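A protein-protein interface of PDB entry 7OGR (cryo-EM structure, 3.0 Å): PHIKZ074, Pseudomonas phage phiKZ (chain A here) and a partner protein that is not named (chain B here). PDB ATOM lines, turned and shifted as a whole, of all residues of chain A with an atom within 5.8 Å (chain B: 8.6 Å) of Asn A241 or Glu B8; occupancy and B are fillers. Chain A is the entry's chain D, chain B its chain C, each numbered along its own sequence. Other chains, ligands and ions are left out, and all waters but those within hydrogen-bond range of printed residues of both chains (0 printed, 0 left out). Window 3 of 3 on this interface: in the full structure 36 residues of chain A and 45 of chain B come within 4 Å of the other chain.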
ATOM      1  N   ILE A 239      13.182 -22.229  15.219  1.00  0.00           N
ATOM      2  CA  ILE A 239      13.074 -21.210  16.255  1.00  0.00           C
ATOM      3  C   ILE A 239      13.463 -19.881  15.626  1.00  0.00           C
ATOM      4  O   ILE A 239      14.629 -19.674  15.267  1.00  0.00           O
ATOM      5  CB  ILE A 239      13.965 -21.534  17.460  1.00  0.00           C
ATOM      6  CG1 ILE A 239      13.567 -22.883  18.064  1.00  0.00           C
ATOM      7  CG2 ILE A 239      13.870 -20.438  18.489  1.00  0.00           C
ATOM      8  CD1 ILE A 239      14.715 -23.661  18.656  1.00  0.00           C
ATOM      9  N   TRP A 240      12.496 -18.976  15.499  1.00  0.00           N
ATOM     10  CA  TRP A 240      12.677 -17.758  14.720  1.00  0.00           C
ATOM     11  C   TRP A 240      12.196 -16.531  15.480  1.00  0.00           C
ATOM     12  O   TRP A 240      11.640 -15.596  14.899  1.00  0.00           O
ATOM     13  CB  TRP A 240      11.959 -17.871  13.381  1.00  0.00           C
ATOM     14  CG  TRP A 240      12.475 -18.975  12.515  1.00  0.00           C
ATOM     15  CD1 TRP A 240      13.739 -19.104  12.014  1.00  0.00           C
ATOM     16  CD2 TRP A 240      11.746 -20.122  12.063  1.00  0.00           C
ATOM     17  NE1 TRP A 240      13.837 -20.254  11.269  1.00  0.00           N
ATOM     18  CE2 TRP A 240      12.628 -20.898  11.285  1.00  0.00           C
ATOM     19  CE3 TRP A 240      10.431 -20.565  12.238  1.00  0.00           C
ATOM     20  CZ2 TRP A 240      12.236 -22.091  10.682  1.00  0.00           C
ATOM     21  CZ3 TRP A 240      10.046 -21.748  11.639  1.00  0.00           C
ATOM     22  CH2 TRP A 240      10.945 -22.498  10.871  1.00  0.00           C
ATOM     23  N   ASN A 241      12.401 -16.513  16.792  1.00  0.00           N
ATOM     24  CA  ASN A 241      12.233 -15.316  17.599  1.00  0.00           C
ATOM     25  C   ASN A 241      13.615 -14.800  17.969  1.00  0.00           C
ATOM     26  O   ASN A 241      14.574 -15.571  18.014  1.00  0.00           O
ATOM     27  CB  ASN A 241      11.420 -15.598  18.865  1.00  0.00           C
ATOM     28  CG  ASN A 241       9.945 -15.788  18.581  1.00  0.00           C
ATOM     29  OD1 ASN A 241       9.439 -15.356  17.547  1.00  0.00           O
ATOM     30  ND2 ASN A 241       9.246 -16.436  19.504  1.00  0.00           N
ATOM     31  N   LEU A 242      13.722 -13.491  18.217  1.00  0.00           N
ATOM     32  CA  LEU A 242      15.026 -12.917  18.547  1.00  0.00           C
ATOM     33  C   LEU A 242      15.524 -13.394  19.905  1.00  0.00           C
ATOM     34  O   LEU A 242      16.714 -13.699  20.059  1.00  0.00           O
ATOM     35  CB  LEU A 242      14.949 -11.390  18.519  1.00  0.00           C
ATOM     36  CG  LEU A 242      16.257 -10.621  18.715  1.00  0.00           C
ATOM     37  CD1 LEU A 242      17.304 -11.050  17.701  1.00  0.00           C
ATOM     38  CD2 LEU A 242      16.019  -9.122  18.638  1.00  0.00           C
ATOM     39  N   TYR A 243      14.609 -13.554  20.860  1.00  0.00           N
ATOM     40  CA  TYR A 243      14.938 -13.912  22.236  1.00  0.00           C
ATOM     41  C   TYR A 243      15.482 -15.335  22.327  1.00  0.00           C
ATOM     42  O   TYR A 243      16.609 -15.558  22.793  1.00  0.00           O
ATOM     43  CB  TYR A 243      13.675 -13.745  23.089  1.00  0.00           C
ATOM     44  CG  TYR A 243      13.777 -14.180  24.529  1.00  0.00           C
ATOM     45  CD1 TYR A 243      14.562 -13.480  25.430  1.00  0.00           C
ATOM     46  CD2 TYR A 243      13.059 -15.276  24.995  1.00  0.00           C
ATOM     47  CE1 TYR A 243      14.651 -13.867  26.747  1.00  0.00           C
ATOM     48  CE2 TYR A 243      13.138 -15.672  26.317  1.00  0.00           C
ATOM     49  CZ  TYR A 243      13.932 -14.957  27.189  1.00  0.00           C
ATOM     50  OH  TYR A 243      14.026 -15.342  28.506  1.00  0.00           O
ATOM     51  N   GLU A 244      14.708 -16.302  21.829  1.00  0.00           N
ATOM     52  CA  GLU A 244      15.067 -17.708  21.969  1.00  0.00           C
ATOM     53  C   GLU A 244      16.257 -18.072  21.084  1.00  0.00           C
ATOM     54  O   GLU A 244      17.106 -18.879  21.483  1.00  0.00           O
ATOM     55  CB  GLU A 244      13.853 -18.574  21.642  1.00  0.00           C
ATOM     56  CG  GLU A 244      12.627 -18.263  22.488  1.00  0.00           C
ATOM     57  CD  GLU A 244      11.365 -18.913  21.952  1.00  0.00           C
ATOM     58  OE1 GLU A 244      11.468 -19.772  21.051  1.00  0.00           O
ATOM     59  OE2 GLU A 244      10.266 -18.561  22.429  1.00  0.00           O
ATOM     60  N   ASN A 245      16.355 -17.466  19.895  1.00  0.00           N
ATOM     61  CA  ASN A 245      17.514 -17.719  19.044  1.00  0.00           C
ATOM     62  C   ASN A 245      18.775 -17.073  19.600  1.00  0.00           C
ATOM     63  O   ASN A 245      19.865 -17.629  19.438  1.00  0.00           O
ATOM     64  CB  ASN A 245      17.264 -17.230  17.617  1.00  0.00           C
ATOM     65  CG  ASN A 245      17.955 -18.086  16.575  1.00  0.00           C
ATOM     66  OD1 ASN A 245      18.926 -18.782  16.867  1.00  0.00           O
ATOM     67  ND2 ASN A 245      17.450 -18.042  15.349  1.00  0.00           N
ATOM     68  N   MET A 246      18.660 -15.933  20.291  1.00  0.00           N
ATOM     69  CA  MET A 246      19.857 -15.387  20.922  1.00  0.00           C
ATOM     70  C   MET A 246      20.295 -16.213  22.127  1.00  0.00           C
ATOM     71  O   MET A 246      21.502 -16.373  22.354  1.00  0.00           O
ATOM     72  CB  MET A 246      19.636 -13.929  21.326  1.00  0.00           C
ATOM     73  CG  MET A 246      19.879 -12.941  20.195  1.00  0.00           C
ATOM     74  SD  MET A 246      20.185 -11.266  20.777  1.00  0.00           S
ATOM     75  CE  MET A 246      21.862 -11.446  21.374  1.00  0.00           C
ATOM     76  N   SER B   2       1.653 -22.814  18.640  1.00  0.00           N
ATOM     77  CA  SER B   2       2.849 -22.355  19.336  1.00  0.00           C
ATOM     78  C   SER B   2       3.668 -21.417  18.454  1.00  0.00           C
ATOM     79  O   SER B   2       4.891 -21.567  18.371  1.00  0.00           O
ATOM     80  CB  SER B   2       3.703 -23.546  19.775  1.00  0.00           C
ATOM     81  OG  SER B   2       4.282 -24.193  18.656  1.00  0.00           O
ATOM     82  N   GLN B   3       2.964 -20.455  17.835  1.00  0.00           N
ATOM     83  CA  GLN B   3       3.471 -19.461  16.866  1.00  0.00           C
ATOM     84  C   GLN B   3       4.393 -20.095  15.811  1.00  0.00           C
ATOM     85  O   GLN B   3       5.517 -19.661  15.563  1.00  0.00           O
ATOM     86  CB  GLN B   3       4.098 -18.232  17.571  1.00  0.00           C
ATOM     87  CG  GLN B   3       5.265 -18.381  18.579  1.00  0.00           C
ATOM     88  CD  GLN B   3       6.640 -18.203  17.966  1.00  0.00           C
ATOM     89  OE1 GLN B   3       6.811 -17.446  17.011  1.00  0.00           O
ATOM     90  NE2 GLN B   3       7.624 -18.913  18.503  1.00  0.00           N
ATOM     91  N   LEU B   4       3.855 -21.121  15.147  1.00  0.00           N
ATOM     92  CA  LEU B   4       4.629 -21.869  14.162  1.00  0.00           C
ATOM     93  C   LEU B   4       4.774 -21.105  12.848  1.00  0.00           C
ATOM     94  O   LEU B   4       5.852 -21.103  12.244  1.00  0.00           O
ATOM     95  CB  LEU B   4       3.977 -23.230  13.910  1.00  0.00           C
ATOM     96  CG  LEU B   4       4.219 -24.340  14.934  1.00  0.00           C
ATOM     97  CD1 LEU B   4       3.592 -25.647  14.466  1.00  0.00           C
ATOM     98  CD2 LEU B   4       5.705 -24.517  15.193  1.00  0.00           C
ATOM     99  N   GLY B   5       3.700 -20.457  12.388  1.00  0.00           N
ATOM    100  CA  GLY B   5       3.709 -19.846  11.071  1.00  0.00           C
ATOM    101  C   GLY B   5       4.360 -18.482  10.990  1.00  0.00           C
ATOM    102  O   GLY B   5       4.653 -18.019   9.884  1.00  0.00           O
ATOM    103  N   ARG B   6       4.594 -17.825  12.123  1.00  0.00           N
ATOM    104  CA  ARG B   6       5.096 -16.459  12.121  1.00  0.00           C
ATOM    105  C   ARG B   6       6.587 -16.415  12.438  1.00  0.00           C
ATOM    106  O   ARG B   6       7.109 -17.230  13.204  1.00  0.00           O
ATOM    107  CB  ARG B   6       4.317 -15.587  13.112  1.00  0.00           C
ATOM    108  CG  ARG B   6       4.410 -16.012  14.567  1.00  0.00           C
ATOM    109  CD  ARG B   6       3.876 -14.926  15.488  1.00  0.00           C
ATOM    110  NE  ARG B   6       4.442 -13.617  15.174  1.00  0.00           N
ATOM    111  CZ  ARG B   6       5.572 -13.146  15.691  1.00  0.00           C
ATOM    112  NH1 ARG B   6       6.266 -13.878  16.553  1.00  0.00           N
ATOM    113  NH2 ARG B   6       6.009 -11.943  15.347  1.00  0.00           N
ATOM    114  N   ARG B   7       7.276 -15.460  11.811  1.00  0.00           N
ATOM    115  CA  ARG B   7       8.707 -15.246  11.990  1.00  0.00           C
ATOM    116  C   ARG B   7       8.960 -13.748  12.083  1.00  0.00           C
ATOM    117  O   ARG B   7       8.367 -12.969  11.333  1.00  0.00           O
ATOM    118  CB  ARG B   7       9.521 -15.852  10.835  1.00  0.00           C
ATOM    119  CG  ARG B   7       9.471 -17.374  10.767  1.00  0.00           C
ATOM    120  CD  ARG B   7       9.772 -17.912   9.384  1.00  0.00           C
ATOM    121  NE  ARG B   7      11.203 -18.072   9.149  1.00  0.00           N
ATOM    122  CZ  ARG B   7      11.719 -18.766   8.140  1.00  0.00           C
ATOM    123  NH1 ARG B   7      13.034 -18.861   8.002  1.00  0.00           N
ATOM    124  NH2 ARG B   7      10.920 -19.373   7.273  1.00  0.00           N
ATOM    125  N   GLU B   8       9.842 -13.343  13.003  1.00  0.00           N
ATOM    126  CA  GLU B   8      10.034 -11.925  13.294  1.00  0.00           C
ATOM    127  C   GLU B   8      11.506 -11.518  13.274  1.00  0.00           C
ATOM    128  O   GLU B   8      11.914 -10.613  14.009  1.00  0.00           O
ATOM    129  CB  GLU B   8       9.391 -11.557  14.634  1.00  0.00           C
ATOM    130  CG  GLU B   8       9.878 -12.371  15.828  1.00  0.00           C
ATOM    131  CD  GLU B   8       9.222 -11.940  17.126  1.00  0.00           C
ATOM    132  OE1 GLU B   8       8.342 -11.055  17.084  1.00  0.00           O
ATOM    133  OE2 GLU B   8       9.594 -12.479  18.189  1.00  0.00           O
ATOM    134  N   ILE B   9      12.315 -12.146  12.425  1.00  0.00           N
ATOM    135  CA  ILE B   9      13.714 -11.770  12.250  1.00  0.00           C
ATOM    136  C   ILE B   9      13.960 -11.558  10.764  1.00  0.00           C
ATOM    137  O   ILE B   9      13.766 -12.480   9.961  1.00  0.00           O
ATOM    138  CB  ILE B   9      14.681 -12.828  12.809  1.00  0.00           C
ATOM    139  CG1 ILE B   9      14.555 -12.937  14.330  1.00  0.00           C
ATOM    140  CG2 ILE B   9      16.117 -12.498  12.424  1.00  0.00           C
ATOM    141  CD1 ILE B   9      15.404 -14.036  14.930  1.00  0.00           C
ATOM    142  N   ASP B  10      14.388 -10.354  10.397  1.00  0.00           N
ATOM    143  CA  ASP B  10      14.633  -9.998   9.011  1.00  0.00           C
ATOM    144  C   ASP B  10      16.128 -10.087   8.703  1.00  0.00           C
ATOM    145  O   ASP B  10      16.930 -10.548   9.520  1.00  0.00           O
ATOM    146  CB  ASP B  10      14.066  -8.607   8.719  1.00  0.00           C
ATOM    147  CG  ASP B  10      14.780  -7.514   9.485  1.00  0.00           C
ATOM    148  OD1 ASP B  10      15.100  -7.730  10.673  1.00  0.00           O
ATOM    149  OD2 ASP B  10      15.016  -6.436   8.903  1.00  0.00           O
ATOM    150  N   LEU B  11      16.510  -9.639   7.505  1.00  0.00           N
ATOM    151  CA  LEU B  11      17.875  -9.787   7.014  1.00  0.00           C
ATOM    152  C   LEU B  11      18.870  -8.855   7.694  1.00  0.00           C
ATOM    153  O   LEU B  11      20.079  -9.076   7.568  1.00  0.00           O
ATOM    154  CB  LEU B  11      17.908  -9.550   5.502  1.00  0.00           C
ATOM    155  CG  LEU B  11      18.909 -10.361   4.677  1.00  0.00           C
ATOM    156  CD1 LEU B  11      18.720 -11.849   4.910  1.00  0.00           C
ATOM    157  CD2 LEU B  11      18.774 -10.026   3.201  1.00  0.00           C
ATOM    158  N   LEU B  13      19.168  -8.281  11.016  1.00  0.00           N
ATOM    159  CA  LEU B  13      19.620  -8.769  12.313  1.00  0.00           C
ATOM    160  C   LEU B  13      20.615  -9.915  12.203  1.00  0.00           C
ATOM    161  O   LEU B  13      21.404 -10.120  13.131  1.00  0.00           O
ATOM    162  CB  LEU B  13      18.423  -9.222  13.160  1.00  0.00           C
ATOM    163  CG  LEU B  13      17.357  -8.167  13.466  1.00  0.00           C
ATOM    164  CD1 LEU B  13      16.006  -8.823  13.709  1.00  0.00           C
ATOM    165  CD2 LEU B  13      17.762  -7.314  14.657  1.00  0.00           C
ATOM    166  N   LEU B  14      20.597 -10.657  11.098  1.00  0.00           N
ATOM    167  CA  LEU B  14      21.549 -11.731  10.844  1.00  0.00           C
ATOM    168  C   LEU B  14      22.632 -11.208   9.908  1.00  0.00           C
ATOM    169  O   LEU B  14      22.332 -10.773   8.792  1.00  0.00           O
ATOM    170  CB  LEU B  14      20.845 -12.940  10.231  1.00  0.00           C
ATOM    171  CG  LEU B  14      19.616 -13.466  10.973  1.00  0.00           C
ATOM    172  CD1 LEU B  14      18.819 -14.403  10.083  1.00  0.00           C
ATOM    173  CD2 LEU B  14      20.019 -14.162  12.263  1.00  0.00           C
ATOM    174  N   TYR B  23      17.675 -21.222   9.066  1.00  0.00           N
ATOM    175  CA  TYR B  23      18.696 -20.993  10.082  1.00  0.00           C
ATOM    176  C   TYR B  23      18.220 -21.409  11.468  1.00  0.00           C
ATOM    177  O   TYR B  23      19.039 -21.783  12.316  1.00  0.00           O
ATOM    178  CB  TYR B  23      19.123 -19.520  10.081  1.00  0.00           C
ATOM    179  CG  TYR B  23      18.030 -18.536  10.461  1.00  0.00           C
ATOM    180  CD1 TYR B  23      17.119 -18.079   9.513  1.00  0.00           C
ATOM    181  CD2 TYR B  23      17.922 -18.049  11.762  1.00  0.00           C
ATOM    182  CE1 TYR B  23      16.123 -17.187   9.851  1.00  0.00           C
ATOM    183  CE2 TYR B  23      16.926 -17.155  12.108  1.00  0.00           C
ATOM    184  CZ  TYR B  23      16.033 -16.728  11.148  1.00  0.00           C
ATOM    185  OH  TYR B  23      15.041 -15.839  11.480  1.00  0.00           O
ATOM    186  N   GLY B  24      16.909 -21.349  11.721  1.00  0.00           N
ATOM    187  CA  GLY B  24      16.387 -21.740  13.017  1.00  0.00           C
ATOM    188  C   GLY B  24      16.299 -23.233  13.229  1.00  0.00           C
ATOM    189  O   GLY B  24      16.172 -23.679  14.374  1.00  0.00           O
ATOM    190  N   VAL B 523      14.544 -14.977   4.992  1.00  0.00           N
ATOM    191  CA  VAL B 523      14.750 -15.393   6.373  1.00  0.00           C
ATOM    192  C   VAL B 523      13.480 -15.271   7.203  1.00  0.00           C
ATOM    193  O   VAL B 523      13.372 -15.905   8.259  1.00  0.00           O
ATOM    194  CB  VAL B 523      15.892 -14.584   7.012  1.00  0.00           C
ATOM    195  CG1 VAL B 523      17.231 -15.015   6.436  1.00  0.00           C
ATOM    196  CG2 VAL B 523      15.669 -13.098   6.795  1.00  0.00           C
ATOM    197  N   ASP B 524      12.510 -14.468   6.758  1.00  0.00           N
ATOM    198  CA  ASP B 524      11.212 -14.336   7.425  1.00  0.00           C
ATOM    199  C   ASP B 524      10.124 -14.631   6.391  1.00  0.00           C
ATOM    200  O   ASP B 524       9.574 -13.729   5.754  1.00  0.00           O
ATOM    201  CB  ASP B 524      11.059 -12.949   8.067  1.00  0.00           C
ATOM    202  CG  ASP B 524      11.552 -11.828   7.171  1.00  0.00           C
ATOM    203  OD1 ASP B 524      12.089 -12.125   6.083  1.00  0.00           O
ATOM    204  OD2 ASP B 524      11.407 -10.649   7.557  1.00  0.00           O
ATOM    205  N   ASP B 525       9.811 -15.914   6.234  1.00  0.00           N
ATOM    206  CA  ASP B 525       8.801 -16.366   5.289  1.00  0.00           C
ATOM    207  C   ASP B 525       7.647 -16.990   6.057  1.00  0.00           C
ATOM    208  O   ASP B 525       7.852 -18.003   6.741  1.00  0.00           O
ATOM    209  CB  ASP B 525       9.398 -17.375   4.308  1.00  0.00           C
ATOM    210  CG  ASP B 525       8.683 -17.387   2.972  1.00  0.00           C
ATOM    211  OD1 ASP B 525       7.787 -16.544   2.765  1.00  0.00           O
ATOM    212  OD2 ASP B 525       9.019 -18.242   2.126  1.00  0.00           O
ATOM    213  N   PRO B 526       6.427 -16.440   5.979  1.00  0.00           N
ATOM    214  CA  PRO B 526       5.313 -16.993   6.766  1.00  0.00           C
ATOM    215  C   PRO B 526       4.826 -18.346   6.265  1.00  0.00           C
ATOM    216  O   PRO B 526       3.753 -18.449   5.663  1.00  0.00           O
ATOM    217  CB  PRO B 526       4.228 -15.919   6.626  1.00  0.00           C
ATOM    218  CG  PRO B 526       4.541 -15.245   5.330  1.00  0.00           C
ATOM    219  CD  PRO B 526       6.038 -15.216   5.258  1.00  0.00           C
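The guanidinium group of Arg B6 is in salt-bridge range of the side-chain carboxylate of Glu B8, 3.0 Å away.
The guanidinium group (NH1) of Arg B7 sits at hydrogen-bond distance from the backbone carbonyl oxygen (O) of Val B523, 3.0 Å away.
The backbone carbonyl oxygen of Asp B525 sits close to the guanidinium group of Arg B7, 3.4 Å away.
The backbone carbonyl oxygen of Ile A239 sits at hydrogen-bond distance from the side-chain amide nitrogen of Asn A245 (3.3 Å).
Of the 8 printed residues of chain A, 5 touch a printed residue of chain B.
Hydrophobic or aromatic side chains of chain A within 4 Å of the printed part of chain B: Trp A240.
Among the printed residues, no Asp or Glu carboxylate lies within 4 Å of a Lys or Arg side-chain nitrogen of the other chain.
Among the printed residues, pairs that only touch across the chains: Trp A240 with Arg B7, Trp A240 with Ile B9, Trp A240 with Tyr B23, Asn A241 with Arg B6, Asn A241 with Ile B9, Leu A242 with Ile B9 and Asn A245 with Tyr B23.
Asn A241 touches just these residues of chain B: Gln B3, Arg B6, Glu B8 and Ile B9.
Of the printed residues of chain B, Leu A242 touches Ile B9 (3.7 Å).
Of the printed residues of chain B, Asn A245 touches Tyr B23 (3.4 Å).
Printed residues of chain A within 4 Å of Arg B6: Asn A241.
Glu B8 touches just these residues of chain A: Trp A240 and Asn A241.
Leu B14 touches none of the printed residues of chain A.
The nearest residue of chain B that does not touch Asn A241 is Arg B7 (5.6 Å).
The nearest residue of chain A that does not touch Glu B8 is Leu A242 (4.3 Å).
The nearest printed residue of chain B that does not touch Asn A245 is Gly B24 (4.5 Å).
NE2 of Gln B3 lies close to ND2 of Asn A241.
The backbone NH (N) of Glu B8 sits at hydrogen-bond distance from the backbone carbonyl oxygen (O) of Trp A240 (3.5 Å).
The side-chain carboxylate of Glu B8 sits close to the side-chain amide oxygen of Asn A241 (3.0 Å).
N of Ile A239 sits at hydrogen-bond distance from O of Gly B24.
NE1 of Trp A240 lies close to N of Gly B24, 3.3 Å away.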
